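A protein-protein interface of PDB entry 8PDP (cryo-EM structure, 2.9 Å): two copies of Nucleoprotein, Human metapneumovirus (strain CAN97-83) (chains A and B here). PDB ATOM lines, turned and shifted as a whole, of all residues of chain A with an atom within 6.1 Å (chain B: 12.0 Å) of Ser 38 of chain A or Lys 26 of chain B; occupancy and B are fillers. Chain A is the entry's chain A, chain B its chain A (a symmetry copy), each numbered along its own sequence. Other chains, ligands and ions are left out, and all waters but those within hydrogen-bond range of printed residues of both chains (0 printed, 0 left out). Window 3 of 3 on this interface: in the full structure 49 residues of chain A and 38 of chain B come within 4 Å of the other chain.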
ATOM      1  N   THR A  36     -35.251   8.095  -5.118  1.00  0.00           N
ATOM      2  CA  THR A  36     -35.579   7.986  -3.711  1.00  0.00           C
ATOM      3  C   THR A  36     -34.903   9.104  -2.929  1.00  0.00           C
ATOM      4  O   THR A  36     -33.688   9.303  -3.067  1.00  0.00           O
ATOM      5  CB  THR A  36     -35.148   6.623  -3.153  1.00  0.00           C
ATOM      6  OG1 THR A  36     -35.504   5.593  -4.082  1.00  0.00           O
ATOM      7  CG2 THR A  36     -35.825   6.354  -1.828  1.00  0.00           C
ATOM      8  N   PRO A  37     -35.642   9.856  -2.118  1.00  0.00           N
ATOM      9  CA  PRO A  37     -35.025  10.944  -1.354  1.00  0.00           C
ATOM     10  C   PRO A  37     -34.096  10.405  -0.281  1.00  0.00           C
ATOM     11  O   PRO A  37     -34.222   9.264   0.166  1.00  0.00           O
ATOM     12  CB  PRO A  37     -36.226  11.671  -0.736  1.00  0.00           C
ATOM     13  CG  PRO A  37     -37.311  10.663  -0.744  1.00  0.00           C
ATOM     14  CD  PRO A  37     -37.101   9.831  -1.959  1.00  0.00           C
ATOM     15  N   SER A  38     -33.148  11.250   0.128  1.00  0.00           N
ATOM     16  CA  SER A  38     -32.131  10.819   1.082  1.00  0.00           C
ATOM     17  C   SER A  38     -32.740  10.402   2.415  1.00  0.00           C
ATOM     18  O   SER A  38     -32.164   9.566   3.122  1.00  0.00           O
ATOM     19  CB  SER A  38     -31.105  11.932   1.287  1.00  0.00           C
ATOM     20  OG  SER A  38     -30.063  11.510   2.146  1.00  0.00           O
ATOM     21  N   SER A  39     -33.902  10.957   2.771  1.00  0.00           N
ATOM     22  CA  SER A  39     -34.538  10.601   4.036  1.00  0.00           C
ATOM     23  C   SER A  39     -34.859   9.115   4.107  1.00  0.00           C
ATOM     24  O   SER A  39     -34.810   8.520   5.190  1.00  0.00           O
ATOM     25  CB  SER A  39     -35.811  11.424   4.234  1.00  0.00           C
ATOM     26  OG  SER A  39     -35.581  12.797   3.974  1.00  0.00           O
ATOM     27  N   LEU A  40     -35.185   8.500   2.975  1.00  0.00           N
ATOM     28  CA  LEU A  40     -35.486   7.077   2.910  1.00  0.00           C
ATOM     29  C   LEU A  40     -34.244   6.207   2.779  1.00  0.00           C
ATOM     30  O   LEU A  40     -34.384   5.005   2.521  1.00  0.00           O
ATOM     31  CB  LEU A  40     -36.436   6.793   1.743  1.00  0.00           C
ATOM     32  CG  LEU A  40     -37.922   7.113   1.902  1.00  0.00           C
ATOM     33  CD1 LEU A  40     -38.184   8.600   1.909  1.00  0.00           C
ATOM     34  CD2 LEU A  40     -38.686   6.467   0.767  1.00  0.00           C
ATOM     35  N   GLN A  41     -33.049   6.777   2.962  1.00  0.00           N
ATOM     36  CA  GLN A  41     -31.819   6.020   2.750  1.00  0.00           C
ATOM     37  C   GLN A  41     -31.802   4.747   3.586  1.00  0.00           C
ATOM     38  O   GLN A  41     -31.591   3.648   3.059  1.00  0.00           O
ATOM     39  CB  GLN A  41     -30.609   6.897   3.072  1.00  0.00           C
ATOM     40  CG  GLN A  41     -29.325   6.451   2.403  1.00  0.00           C
ATOM     41  CD  GLN A  41     -28.098   7.077   3.024  1.00  0.00           C
ATOM     42  OE1 GLN A  41     -27.920   7.043   4.239  1.00  0.00           O
ATOM     43  NE2 GLN A  41     -27.246   7.659   2.191  1.00  0.00           N
ATOM     44  N   GLN A  42     -32.068   4.870   4.888  1.00  0.00           N
ATOM     45  CA  GLN A  42     -32.183   3.687   5.734  1.00  0.00           C
ATOM     46  C   GLN A  42     -33.167   2.689   5.137  1.00  0.00           C
ATOM     47  O   GLN A  42     -32.831   1.518   4.920  1.00  0.00           O
ATOM     48  CB  GLN A  42     -32.627   4.093   7.140  1.00  0.00           C
ATOM     49  CG  GLN A  42     -31.636   4.946   7.914  1.00  0.00           C
ATOM     50  CD  GLN A  42     -30.325   4.237   8.180  1.00  0.00           C
ATOM     51  OE1 GLN A  42     -29.292   4.574   7.602  1.00  0.00           O
ATOM     52  NE2 GLN A  42     -30.357   3.250   9.068  1.00  0.00           N
ATOM     53  N   TYR A  69     -30.555   3.660  -4.266  1.00  0.00           N
ATOM     54  CA  TYR A  69     -29.582   4.012  -3.237  1.00  0.00           C
ATOM     55  C   TYR A  69     -28.637   5.105  -3.718  1.00  0.00           C
ATOM     56  O   TYR A  69     -28.260   5.992  -2.943  1.00  0.00           O
ATOM     57  CB  TYR A  69     -28.780   2.795  -2.791  1.00  0.00           C
ATOM     58  CG  TYR A  69     -27.739   3.176  -1.769  1.00  0.00           C
ATOM     59  CD1 TYR A  69     -28.090   3.406  -0.449  1.00  0.00           C
ATOM     60  CD2 TYR A  69     -26.409   3.338  -2.129  1.00  0.00           C
ATOM     61  CE1 TYR A  69     -27.146   3.770   0.484  1.00  0.00           C
ATOM     62  CE2 TYR A  69     -25.462   3.704  -1.204  1.00  0.00           C
ATOM     63  CZ  TYR A  69     -25.833   3.917   0.101  1.00  0.00           C
ATOM     64  OH  TYR A  69     -24.884   4.280   1.028  1.00  0.00           O
ATOM     65  N   SER A  71     -29.433   7.433  -5.737  1.00  0.00           N
ATOM     66  CA  SER A  71     -30.237   8.646  -5.643  1.00  0.00           C
ATOM     67  C   SER A  71     -30.296   9.165  -4.213  1.00  0.00           C
ATOM     68  O   SER A  71     -30.227  10.377  -3.983  1.00  0.00           O
ATOM     69  CB  SER A  71     -31.644   8.379  -6.167  1.00  0.00           C
ATOM     70  OG  SER A  71     -32.491   9.464  -5.857  1.00  0.00           O
ATOM     71  N   THR A  72     -30.444   8.265  -3.243  1.00  0.00           N
ATOM     72  CA  THR A  72     -30.440   8.691  -1.846  1.00  0.00           C
ATOM     73  C   THR A  72     -29.099   9.302  -1.465  1.00  0.00           C
ATOM     74  O   THR A  72     -29.046  10.303  -0.743  1.00  0.00           O
ATOM     75  CB  THR A  72     -30.757   7.515  -0.924  1.00  0.00           C
ATOM     76  OG1 THR A  72     -29.769   6.495  -1.098  1.00  0.00           O
ATOM     77  CG2 THR A  72     -32.120   6.944  -1.240  1.00  0.00           C
ATOM     78  N   ALA A  73     -28.003   8.707  -1.935  1.00  0.00           N
ATOM     79  CA  ALA A  73     -26.675   9.208  -1.596  1.00  0.00           C
ATOM     80  C   ALA A  73     -26.429  10.588  -2.194  1.00  0.00           C
ATOM     81  O   ALA A  73     -25.872  11.469  -1.531  1.00  0.00           O
ATOM     82  CB  ALA A  73     -25.604   8.222  -2.058  1.00  0.00           C
ATOM     83  N   LEU A  74     -26.813  10.791  -3.454  1.00  0.00           N
ATOM     84  CA  LEU A  74     -26.602  12.096  -4.078  1.00  0.00           C
ATOM     85  C   LEU A  74     -27.703  13.090  -3.723  1.00  0.00           C
ATOM     86  O   LEU A  74     -27.423  14.271  -3.488  1.00  0.00           O
ATOM     87  CB  LEU A  74     -26.493  11.947  -5.594  1.00  0.00           C
ATOM     88  CG  LEU A  74     -25.427  10.989  -6.120  1.00  0.00           C
ATOM     89  CD1 LEU A  74     -25.675  10.683  -7.578  1.00  0.00           C
ATOM     90  CD2 LEU A  74     -24.040  11.569  -5.930  1.00  0.00           C
ATOM     91  N   GLY A  75     -28.946  12.643  -3.680  1.00  0.00           N
ATOM     92  CA  GLY A  75     -30.079  13.530  -3.477  1.00  0.00           C
ATOM     93  C   GLY A  75     -30.961  13.524  -4.714  1.00  0.00           C
ATOM     94  O   GLY A  75     -30.476  13.420  -5.845  1.00  0.00           O
ATOM     95  N   SER A  76     -32.272  13.641  -4.496  1.00  0.00           N
ATOM     96  CA  SER A  76     -33.227  13.504  -5.593  1.00  0.00           C
ATOM     97  C   SER A  76     -33.093  14.637  -6.607  1.00  0.00           C
ATOM     98  O   SER A  76     -33.069  14.397  -7.821  1.00  0.00           O
ATOM     99  CB  SER A  76     -34.648  13.444  -5.033  1.00  0.00           C
ATOM    100  OG  SER A  76     -35.011  14.671  -4.423  1.00  0.00           O
ATOM    101  N   SER B  21     -15.633  16.845  -8.891  1.00  0.00           N
ATOM    102  CA  SER B  21     -17.038  16.473  -8.782  1.00  0.00           C
ATOM    103  C   SER B  21     -17.807  17.588  -8.091  1.00  0.00           C
ATOM    104  O   SER B  21     -17.327  18.164  -7.109  1.00  0.00           O
ATOM    105  CB  SER B  21     -17.207  15.167  -8.008  1.00  0.00           C
ATOM    106  OG  SER B  21     -18.573  14.932  -7.721  1.00  0.00           O
ATOM    107  N   GLN B  22     -18.998  17.890  -8.605  1.00  0.00           N
ATOM    108  CA  GLN B  22     -19.860  18.918  -8.043  1.00  0.00           C
ATOM    109  C   GLN B  22     -20.954  18.349  -7.149  1.00  0.00           C
ATOM    110  O   GLN B  22     -21.839  19.094  -6.721  1.00  0.00           O
ATOM    111  CB  GLN B  22     -20.488  19.758  -9.161  1.00  0.00           C
ATOM    112  CG  GLN B  22     -19.563  20.078 -10.335  1.00  0.00           C
ATOM    113  CD  GLN B  22     -19.439  18.947 -11.339  1.00  0.00           C
ATOM    114  OE1 GLN B  22     -19.702  17.786 -11.023  1.00  0.00           O
ATOM    115  NE2 GLN B  22     -19.040  19.283 -12.560  1.00  0.00           N
ATOM    116  N   TYR B  23     -20.913  17.053  -6.858  1.00  0.00           N
ATOM    117  CA  TYR B  23     -21.904  16.396  -6.018  1.00  0.00           C
ATOM    118  C   TYR B  23     -21.195  15.713  -4.860  1.00  0.00           C
ATOM    119  O   TYR B  23     -20.179  15.042  -5.061  1.00  0.00           O
ATOM    120  CB  TYR B  23     -22.718  15.381  -6.822  1.00  0.00           C
ATOM    121  CG  TYR B  23     -23.259  15.930  -8.120  1.00  0.00           C
ATOM    122  CD1 TYR B  23     -24.486  16.571  -8.165  1.00  0.00           C
ATOM    123  CD2 TYR B  23     -22.535  15.821  -9.296  1.00  0.00           C
ATOM    124  CE1 TYR B  23     -24.983  17.075  -9.346  1.00  0.00           C
ATOM    125  CE2 TYR B  23     -23.021  16.327 -10.481  1.00  0.00           C
ATOM    126  CZ  TYR B  23     -24.245  16.954 -10.499  1.00  0.00           C
ATOM    127  OH  TYR B  23     -24.735  17.458 -11.680  1.00  0.00           O
ATOM    128  N   THR B  24     -21.722  15.896  -3.656  1.00  0.00           N
ATOM    129  CA  THR B  24     -21.159  15.291  -2.460  1.00  0.00           C
ATOM    130  C   THR B  24     -21.977  14.074  -2.053  1.00  0.00           C
ATOM    131  O   THR B  24     -23.203  14.059  -2.171  1.00  0.00           O
ATOM    132  CB  THR B  24     -21.118  16.293  -1.305  1.00  0.00           C
ATOM    133  OG1 THR B  24     -22.449  16.711  -0.985  1.00  0.00           O
ATOM    134  CG2 THR B  24     -20.293  17.509  -1.688  1.00  0.00           C
ATOM    135  N   ILE B  25     -21.282  13.050  -1.572  1.00  0.00           N
ATOM    136  CA  ILE B  25     -21.943  11.843  -1.098  1.00  0.00           C
ATOM    137  C   ILE B  25     -22.482  12.096   0.301  1.00  0.00           C
ATOM    138  O   ILE B  25     -21.823  12.729   1.133  1.00  0.00           O
ATOM    139  CB  ILE B  25     -20.973  10.648  -1.118  1.00  0.00           C
ATOM    140  CG1 ILE B  25     -20.447  10.403  -2.531  1.00  0.00           C
ATOM    141  CG2 ILE B  25     -21.659   9.392  -0.625  1.00  0.00           C
ATOM    142  CD1 ILE B  25     -21.520  10.068  -3.535  1.00  0.00           C
ATOM    143  N   LYS B  26     -23.687  11.600   0.566  1.00  0.00           N
ATOM    144  CA  LYS B  26     -24.334  11.741   1.863  1.00  0.00           C
ATOM    145  C   LYS B  26     -24.454  10.362   2.489  1.00  0.00           C
ATOM    146  O   LYS B  26     -25.121   9.483   1.934  1.00  0.00           O
ATOM    147  CB  LYS B  26     -25.711  12.390   1.718  1.00  0.00           C
ATOM    148  CG  LYS B  26     -25.669  13.847   1.297  1.00  0.00           C
ATOM    149  CD  LYS B  26     -27.068  14.402   1.103  1.00  0.00           C
ATOM    150  CE  LYS B  26     -27.798  14.559   2.427  1.00  0.00           C
ATOM    151  NZ  LYS B  26     -27.192  15.620   3.273  1.00  0.00           N
ATOM    152  N   ARG B  27     -23.812  10.172   3.636  1.00  0.00           N
ATOM    153  CA  ARG B  27     -23.850   8.904   4.344  1.00  0.00           C
ATOM    154  C   ARG B  27     -24.139   9.150   5.816  1.00  0.00           C
ATOM    155  O   ARG B  27     -23.834  10.219   6.353  1.00  0.00           O
ATOM    156  CB  ARG B  27     -22.534   8.136   4.198  1.00  0.00           C
ATOM    157  CG  ARG B  27     -21.305   8.975   4.468  1.00  0.00           C
ATOM    158  CD  ARG B  27     -20.032   8.209   4.178  1.00  0.00           C
ATOM    159  NE  ARG B  27     -19.869   7.928   2.759  1.00  0.00           N
ATOM    160  CZ  ARG B  27     -18.834   8.340   2.036  1.00  0.00           C
ATOM    161  NH1 ARG B  27     -17.874   9.056   2.599  1.00  0.00           N
ATOM    162  NH2 ARG B  27     -18.761   8.039   0.750  1.00  0.00           N
ATOM    163  N   ASP B  28     -24.733   8.144   6.458  1.00  0.00           N
ATOM    164  CA  ASP B  28     -25.039   8.178   7.888  1.00  0.00           C
ATOM    165  C   ASP B  28     -26.002   9.317   8.220  1.00  0.00           C
ATOM    166  O   ASP B  28     -25.765  10.123   9.121  1.00  0.00           O
ATOM    167  CB  ASP B  28     -23.755   8.283   8.717  1.00  0.00           C
ATOM    168  CG  ASP B  28     -22.912   7.025   8.651  1.00  0.00           C
ATOM    169  OD1 ASP B  28     -23.482   5.929   8.472  1.00  0.00           O
ATOM    170  OD2 ASP B  28     -21.675   7.134   8.776  1.00  0.00           O
ATOM    171  N   VAL B  29     -27.107   9.376   7.473  1.00  0.00           N
ATOM    172  CA  VAL B  29     -28.063  10.466   7.642  1.00  0.00           C
ATOM    173  C   VAL B  29     -28.812  10.341   8.965  1.00  0.00           C
ATOM    174  O   VAL B  29     -29.111  11.346   9.620  1.00  0.00           O
ATOM    175  CB  VAL B  29     -29.022  10.526   6.439  1.00  0.00           C
ATOM    176  CG1 VAL B  29     -28.246  10.808   5.168  1.00  0.00           C
ATOM    177  CG2 VAL B  29     -29.789   9.224   6.299  1.00  0.00           C
ATOM    178  N   GLY B  30     -29.130   9.119   9.378  1.00  0.00           N
ATOM    179  CA  GLY B  30     -29.907   8.887  10.576  1.00  0.00           C
ATOM    180  C   GLY B  30     -29.130   8.450  11.797  1.00  0.00           C
ATOM    181  O   GLY B  30     -29.746   8.010  12.774  1.00  0.00           O
ATOM    182  N   THR B  31     -27.807   8.557  11.785  1.00  0.00           N
ATOM    183  CA  THR B  31     -26.980   8.118  12.898  1.00  0.00           C
ATOM    184  C   THR B  31     -26.606   9.296  13.791  1.00  0.00           C
ATOM    185  O   THR B  31     -26.700  10.461  13.400  1.00  0.00           O
ATOM    186  CB  THR B  31     -25.715   7.423  12.391  1.00  0.00           C
ATOM    187  OG1 THR B  31     -24.879   8.376  11.723  1.00  0.00           O
ATOM    188  CG2 THR B  31     -26.076   6.312  11.421  1.00  0.00           C
ATOM    189  N   GLN B  80     -18.252  18.973  15.492  1.00  0.00           N
ATOM    190  CA  GLN B  80     -19.336  18.944  14.510  1.00  0.00           C
ATOM    191  C   GLN B  80     -18.844  19.356  13.133  1.00  0.00           C
ATOM    192  O   GLN B  80     -19.176  18.725  12.123  1.00  0.00           O
ATOM    193  CB  GLN B  80     -20.486  19.848  14.958  1.00  0.00           C
ATOM    194  CG  GLN B  80     -21.715  19.859  14.029  1.00  0.00           C
ATOM    195  CD  GLN B  80     -22.168  18.492  13.542  1.00  0.00           C
ATOM    196  OE1 GLN B  80     -22.146  17.520  14.297  1.00  0.00           O
ATOM    197  NE2 GLN B  80     -22.525  18.397  12.275  1.00  0.00           N
ATOM    198  N   LEU B  83     -16.667  16.511  11.650  1.00  0.00           N
ATOM    199  CA  LEU B  83     -17.458  15.380  11.183  1.00  0.00           C
ATOM    200  C   LEU B  83     -18.224  15.733   9.916  1.00  0.00           C
ATOM    201  O   LEU B  83     -18.330  14.910   9.000  1.00  0.00           O
ATOM    202  CB  LEU B  83     -18.411  14.921  12.284  1.00  0.00           C
ATOM    203  CG  LEU B  83     -17.745  14.332  13.527  1.00  0.00           C
ATOM    204  CD1 LEU B  83     -18.756  13.596  14.381  1.00  0.00           C
ATOM    205  CD2 LEU B  83     -16.600  13.416  13.147  1.00  0.00           C
ATOM    206  N   ARG B  84     -18.766  16.950   9.845  1.00  0.00           N
ATOM    207  CA  ARG B  84     -19.480  17.373   8.647  1.00  0.00           C
ATOM    208  C   ARG B  84     -18.553  17.454   7.438  1.00  0.00           C
ATOM    209  O   ARG B  84     -18.920  17.027   6.339  1.00  0.00           O
ATOM    210  CB  ARG B  84     -20.165  18.713   8.905  1.00  0.00           C
ATOM    211  CG  ARG B  84     -21.278  19.044   7.934  1.00  0.00           C
ATOM    212  CD  ARG B  84     -21.669  20.507   8.047  1.00  0.00           C
ATOM    213  NE  ARG B  84     -21.649  20.967   9.433  1.00  0.00           N
ATOM    214  CZ  ARG B  84     -20.874  21.945   9.886  1.00  0.00           C
ATOM    215  NH1 ARG B  84     -20.041  22.568   9.066  1.00  0.00           N
ATOM    216  NH2 ARG B  84     -20.928  22.295  11.164  1.00  0.00           N
ATOM    217  N   ASN B  85     -17.343  17.988   7.623  1.00  0.00           N
ATOM    218  CA  ASN B  85     -16.395  18.061   6.517  1.00  0.00           C
ATOM    219  C   ASN B  85     -15.863  16.698   6.098  1.00  0.00           C
ATOM    220  O   ASN B  85     -15.307  16.579   5.003  1.00  0.00           O
ATOM    221  CB  ASN B  85     -15.225  18.975   6.879  1.00  0.00           C
ATOM    222  CG  ASN B  85     -15.648  20.406   7.081  1.00  0.00           C
ATOM    223  OD1 ASN B  85     -16.740  20.682   7.570  1.00  0.00           O
ATOM    224  ND2 ASN B  85     -14.777  21.335   6.710  1.00  0.00           N
ATOM    225  N   SER B  86     -16.012  15.673   6.934  1.00  0.00           N
ATOM    226  CA  SER B  86     -15.533  14.345   6.572  1.00  0.00           C
ATOM    227  C   SER B  86     -16.466  13.620   5.614  1.00  0.00           C
ATOM    228  O   SER B  86     -16.137  12.516   5.171  1.00  0.00           O
ATOM    229  CB  SER B  86     -15.329  13.491   7.824  1.00  0.00           C
ATOM    230  OG  SER B  86     -16.567  13.127   8.403  1.00  0.00           O
ATOM    231  N   GLY B  87     -17.614  14.205   5.288  1.00  0.00           N
ATOM    232  CA  GLY B  87     -18.577  13.565   4.424  1.00  0.00           C
ATOM    233  C   GLY B  87     -19.665  12.790   5.130  1.00  0.00           C
ATOM    234  O   GLY B  87     -20.345  11.991   4.480  1.00  0.00           O
ATOM    235  N   SER B  88     -19.851  12.995   6.429  1.00  0.00           N
ATOM    236  CA  SER B  88     -20.844  12.273   7.208  1.00  0.00           C
ATOM    237  C   SER B  88     -21.918  13.229   7.706  1.00  0.00           C
ATOM    238  O   SER B  88     -21.621  14.359   8.105  1.00  0.00           O
ATOM    239  CB  SER B  88     -20.195  11.561   8.396  1.00  0.00           C
ATOM    240  OG  SER B  88     -21.160  10.864   9.161  1.00  0.00           O
ATOM    241  N   GLU B  89     -23.169  12.768   7.678  1.00  0.00           N
ATOM    242  CA  GLU B  89     -24.304  13.521   8.198  1.00  0.00           C
ATOM    243  C   GLU B  89     -24.655  13.121   9.626  1.00  0.00           C
ATOM    244  O   GLU B  89     -25.808  13.259  10.043  1.00  0.00           O
ATOM    245  CB  GLU B  89     -25.519  13.351   7.287  1.00  0.00           C
ATOM    246  CG  GLU B  89     -25.285  13.790   5.856  1.00  0.00           C
ATOM    247  CD  GLU B  89     -25.081  15.286   5.737  1.00  0.00           C
ATOM    248  OE1 GLU B  89     -24.272  15.713   4.887  1.00  0.00           O
ATOM    249  OE2 GLU B  89     -25.727  16.035   6.496  1.00  0.00           O
ATOM    250  N   VAL B  90     -23.677  12.625  10.382  1.00  0.00           N
ATOM    251  CA  VAL B  90     -23.921  12.203  11.754  1.00  0.00           C
ATOM    252  C   VAL B  90     -24.200  13.420  12.626  1.00  0.00           C
ATOM    253  O   VAL B  90     -23.566  14.473  12.484  1.00  0.00           O
ATOM    254  CB  VAL B  90     -22.729  11.383  12.275  1.00  0.00           C
ATOM    255  CG1 VAL B  90     -21.476  12.239  12.355  1.00  0.00           C
ATOM    256  CG2 VAL B  90     -23.047  10.767  13.619  1.00  0.00           C
ATOM    257  N   GLN B  91     -25.179  13.289  13.515  1.00  0.00           N
ATOM    258  CA  GLN B  91     -25.596  14.375  14.390  1.00  0.00           C
ATOM    259  C   GLN B  91     -25.022  14.159  15.785  1.00  0.00           C
ATOM    260  O   GLN B  91     -25.224  13.102  16.388  1.00  0.00           O
ATOM    261  CB  GLN B  91     -27.119  14.482  14.445  1.00  0.00           C
ATOM    262  CG  GLN B  91     -27.724  15.305  13.320  1.00  0.00           C
ATOM    263  CD  GLN B  91     -26.885  16.516  12.963  1.00  0.00           C
ATOM    264  OE1 GLN B  91     -26.343  16.606  11.863  1.00  0.00           O
ATOM    265  NE2 GLN B  91     -26.776  17.458  13.893  1.00  0.00           N
ATOM    266  N   TYR B 219     -15.637   8.284  10.451  1.00  0.00           N
ATOM    267  CA  TYR B 219     -15.417   9.710  10.675  1.00  0.00           C
ATOM    268  C   TYR B 219     -14.552   9.977  11.900  1.00  0.00           C
ATOM    269  O   TYR B 219     -13.938  11.050  12.006  1.00  0.00           O
ATOM    270  CB  TYR B 219     -16.757  10.432  10.802  1.00  0.00           C
ATOM    271  CG  TYR B 219     -17.756   9.759  11.714  1.00  0.00           C
ATOM    272  CD1 TYR B 219     -17.766  10.014  13.074  1.00  0.00           C
ATOM    273  CD2 TYR B 219     -18.699   8.878  11.209  1.00  0.00           C
ATOM    274  CE1 TYR B 219     -18.679   9.406  13.905  1.00  0.00           C
ATOM    275  CE2 TYR B 219     -19.615   8.267  12.034  1.00  0.00           C
ATOM    276  CZ  TYR B 219     -19.600   8.534  13.379  1.00  0.00           C
ATOM    277  OH  TYR B 219     -20.513   7.926  14.205  1.00  0.00           O
ATOM    278  N   PRO B 308     -12.040   6.612  -0.467  1.00  0.00           N
ATOM    279  CA  PRO B 308     -12.156   5.787  -1.676  1.00  0.00           C
ATOM    280  C   PRO B 308     -11.159   6.156  -2.754  1.00  0.00           C
ATOM    281  O   PRO B 308     -10.838   5.312  -3.596  1.00  0.00           O
ATOM    282  CB  PRO B 308     -13.598   6.038  -2.130  1.00  0.00           C
ATOM    283  CG  PRO B 308     -14.299   6.515  -0.910  1.00  0.00           C
ATOM    284  CD  PRO B 308     -13.292   7.325  -0.178  1.00  0.00           C
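Ser 38 of chain A touches Lys 26 of chain B.
Ser 38 of chain A touches Val 29 of chain B.
OE1 of Gln 41 of chain A touches CG2 of Val 29 of chain B, at 3.5 Å.
Thr 24 of chain B touches Ala 73 of chain A (O to O, 3.8 Å).
C of Ile 25 of chain B touches O of Ala 73 of chain A (3.9 Å).
Leu 74 of chain A touches Ile 25 of chain B.
No position is printed for both chains.
Of chain B, only Lys 26 (3.8 Å) and Val 29 (3.6 Å) come within 4 Å of Ser 38 of chain A.
Lys 26 of chain B touches just these residues of chain A: Ser 38, Gln 41 and Ala 73.
No residue of chain B comes within 4 Å of Pro 37 of chain A.
No residue of chain B comes within 4 Å of Leu 40 of chain A.
Gln 41 of chain A touches two residues of chain B.
No residue of chain B comes within 4 Å of Thr 72 of chain A.
No residue of chain B comes within 4 Å of Gly 75 of chain A.
Printed residues of chain A within 4 Å of Val 29 of chain B: Ser 38 and Gln 41.
Of the printed residues of chain A, Thr 24 of chain B touches Ala 73.
Of the printed residues of chain A, Ile 25 of chain B touches Ala 73 and Leu 74.
Of the printed residues of chain B, Leu 74 of chain A touches Ile 25 (3.8 Å).
Ser 86 of chain B touches none of the printed residues of chain A.
The nearest residue of chain A that does not touch Lys 26 of chain B is Leu 74 of chain A (4.6 Å).
OG of Ser 38 of chain A is in hydrogen-bond range of O of Thr 72 of chain A (3.3 Å).
OE1 of Glu 89 of chain B is in salt-bridge range of NZ of Lys 26 of chain B (3.3 Å).
Hydrophobic or aromatic side chains of chain A within 4 Å of the printed part of chain B: Leu 74.
Of the 23 printed residues of chain B, 4 touch a printed residue of chain A.
Among the printed residues, 8 pairs touch across the chains.
Among the printed residues, no Asp or Glu carboxylate lies within 4 Å of a Lys or Arg side-chain nitrogen of the other chain.
NE2 of Gln 41 of chain A sits at hydrogen-bond distance from O of Lys 26 of chain B, 2.8 Å away.
O of Ala 73 of chain A sits at hydrogen-bond distance from N of Lys 26 of chain B (3.0 Å).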
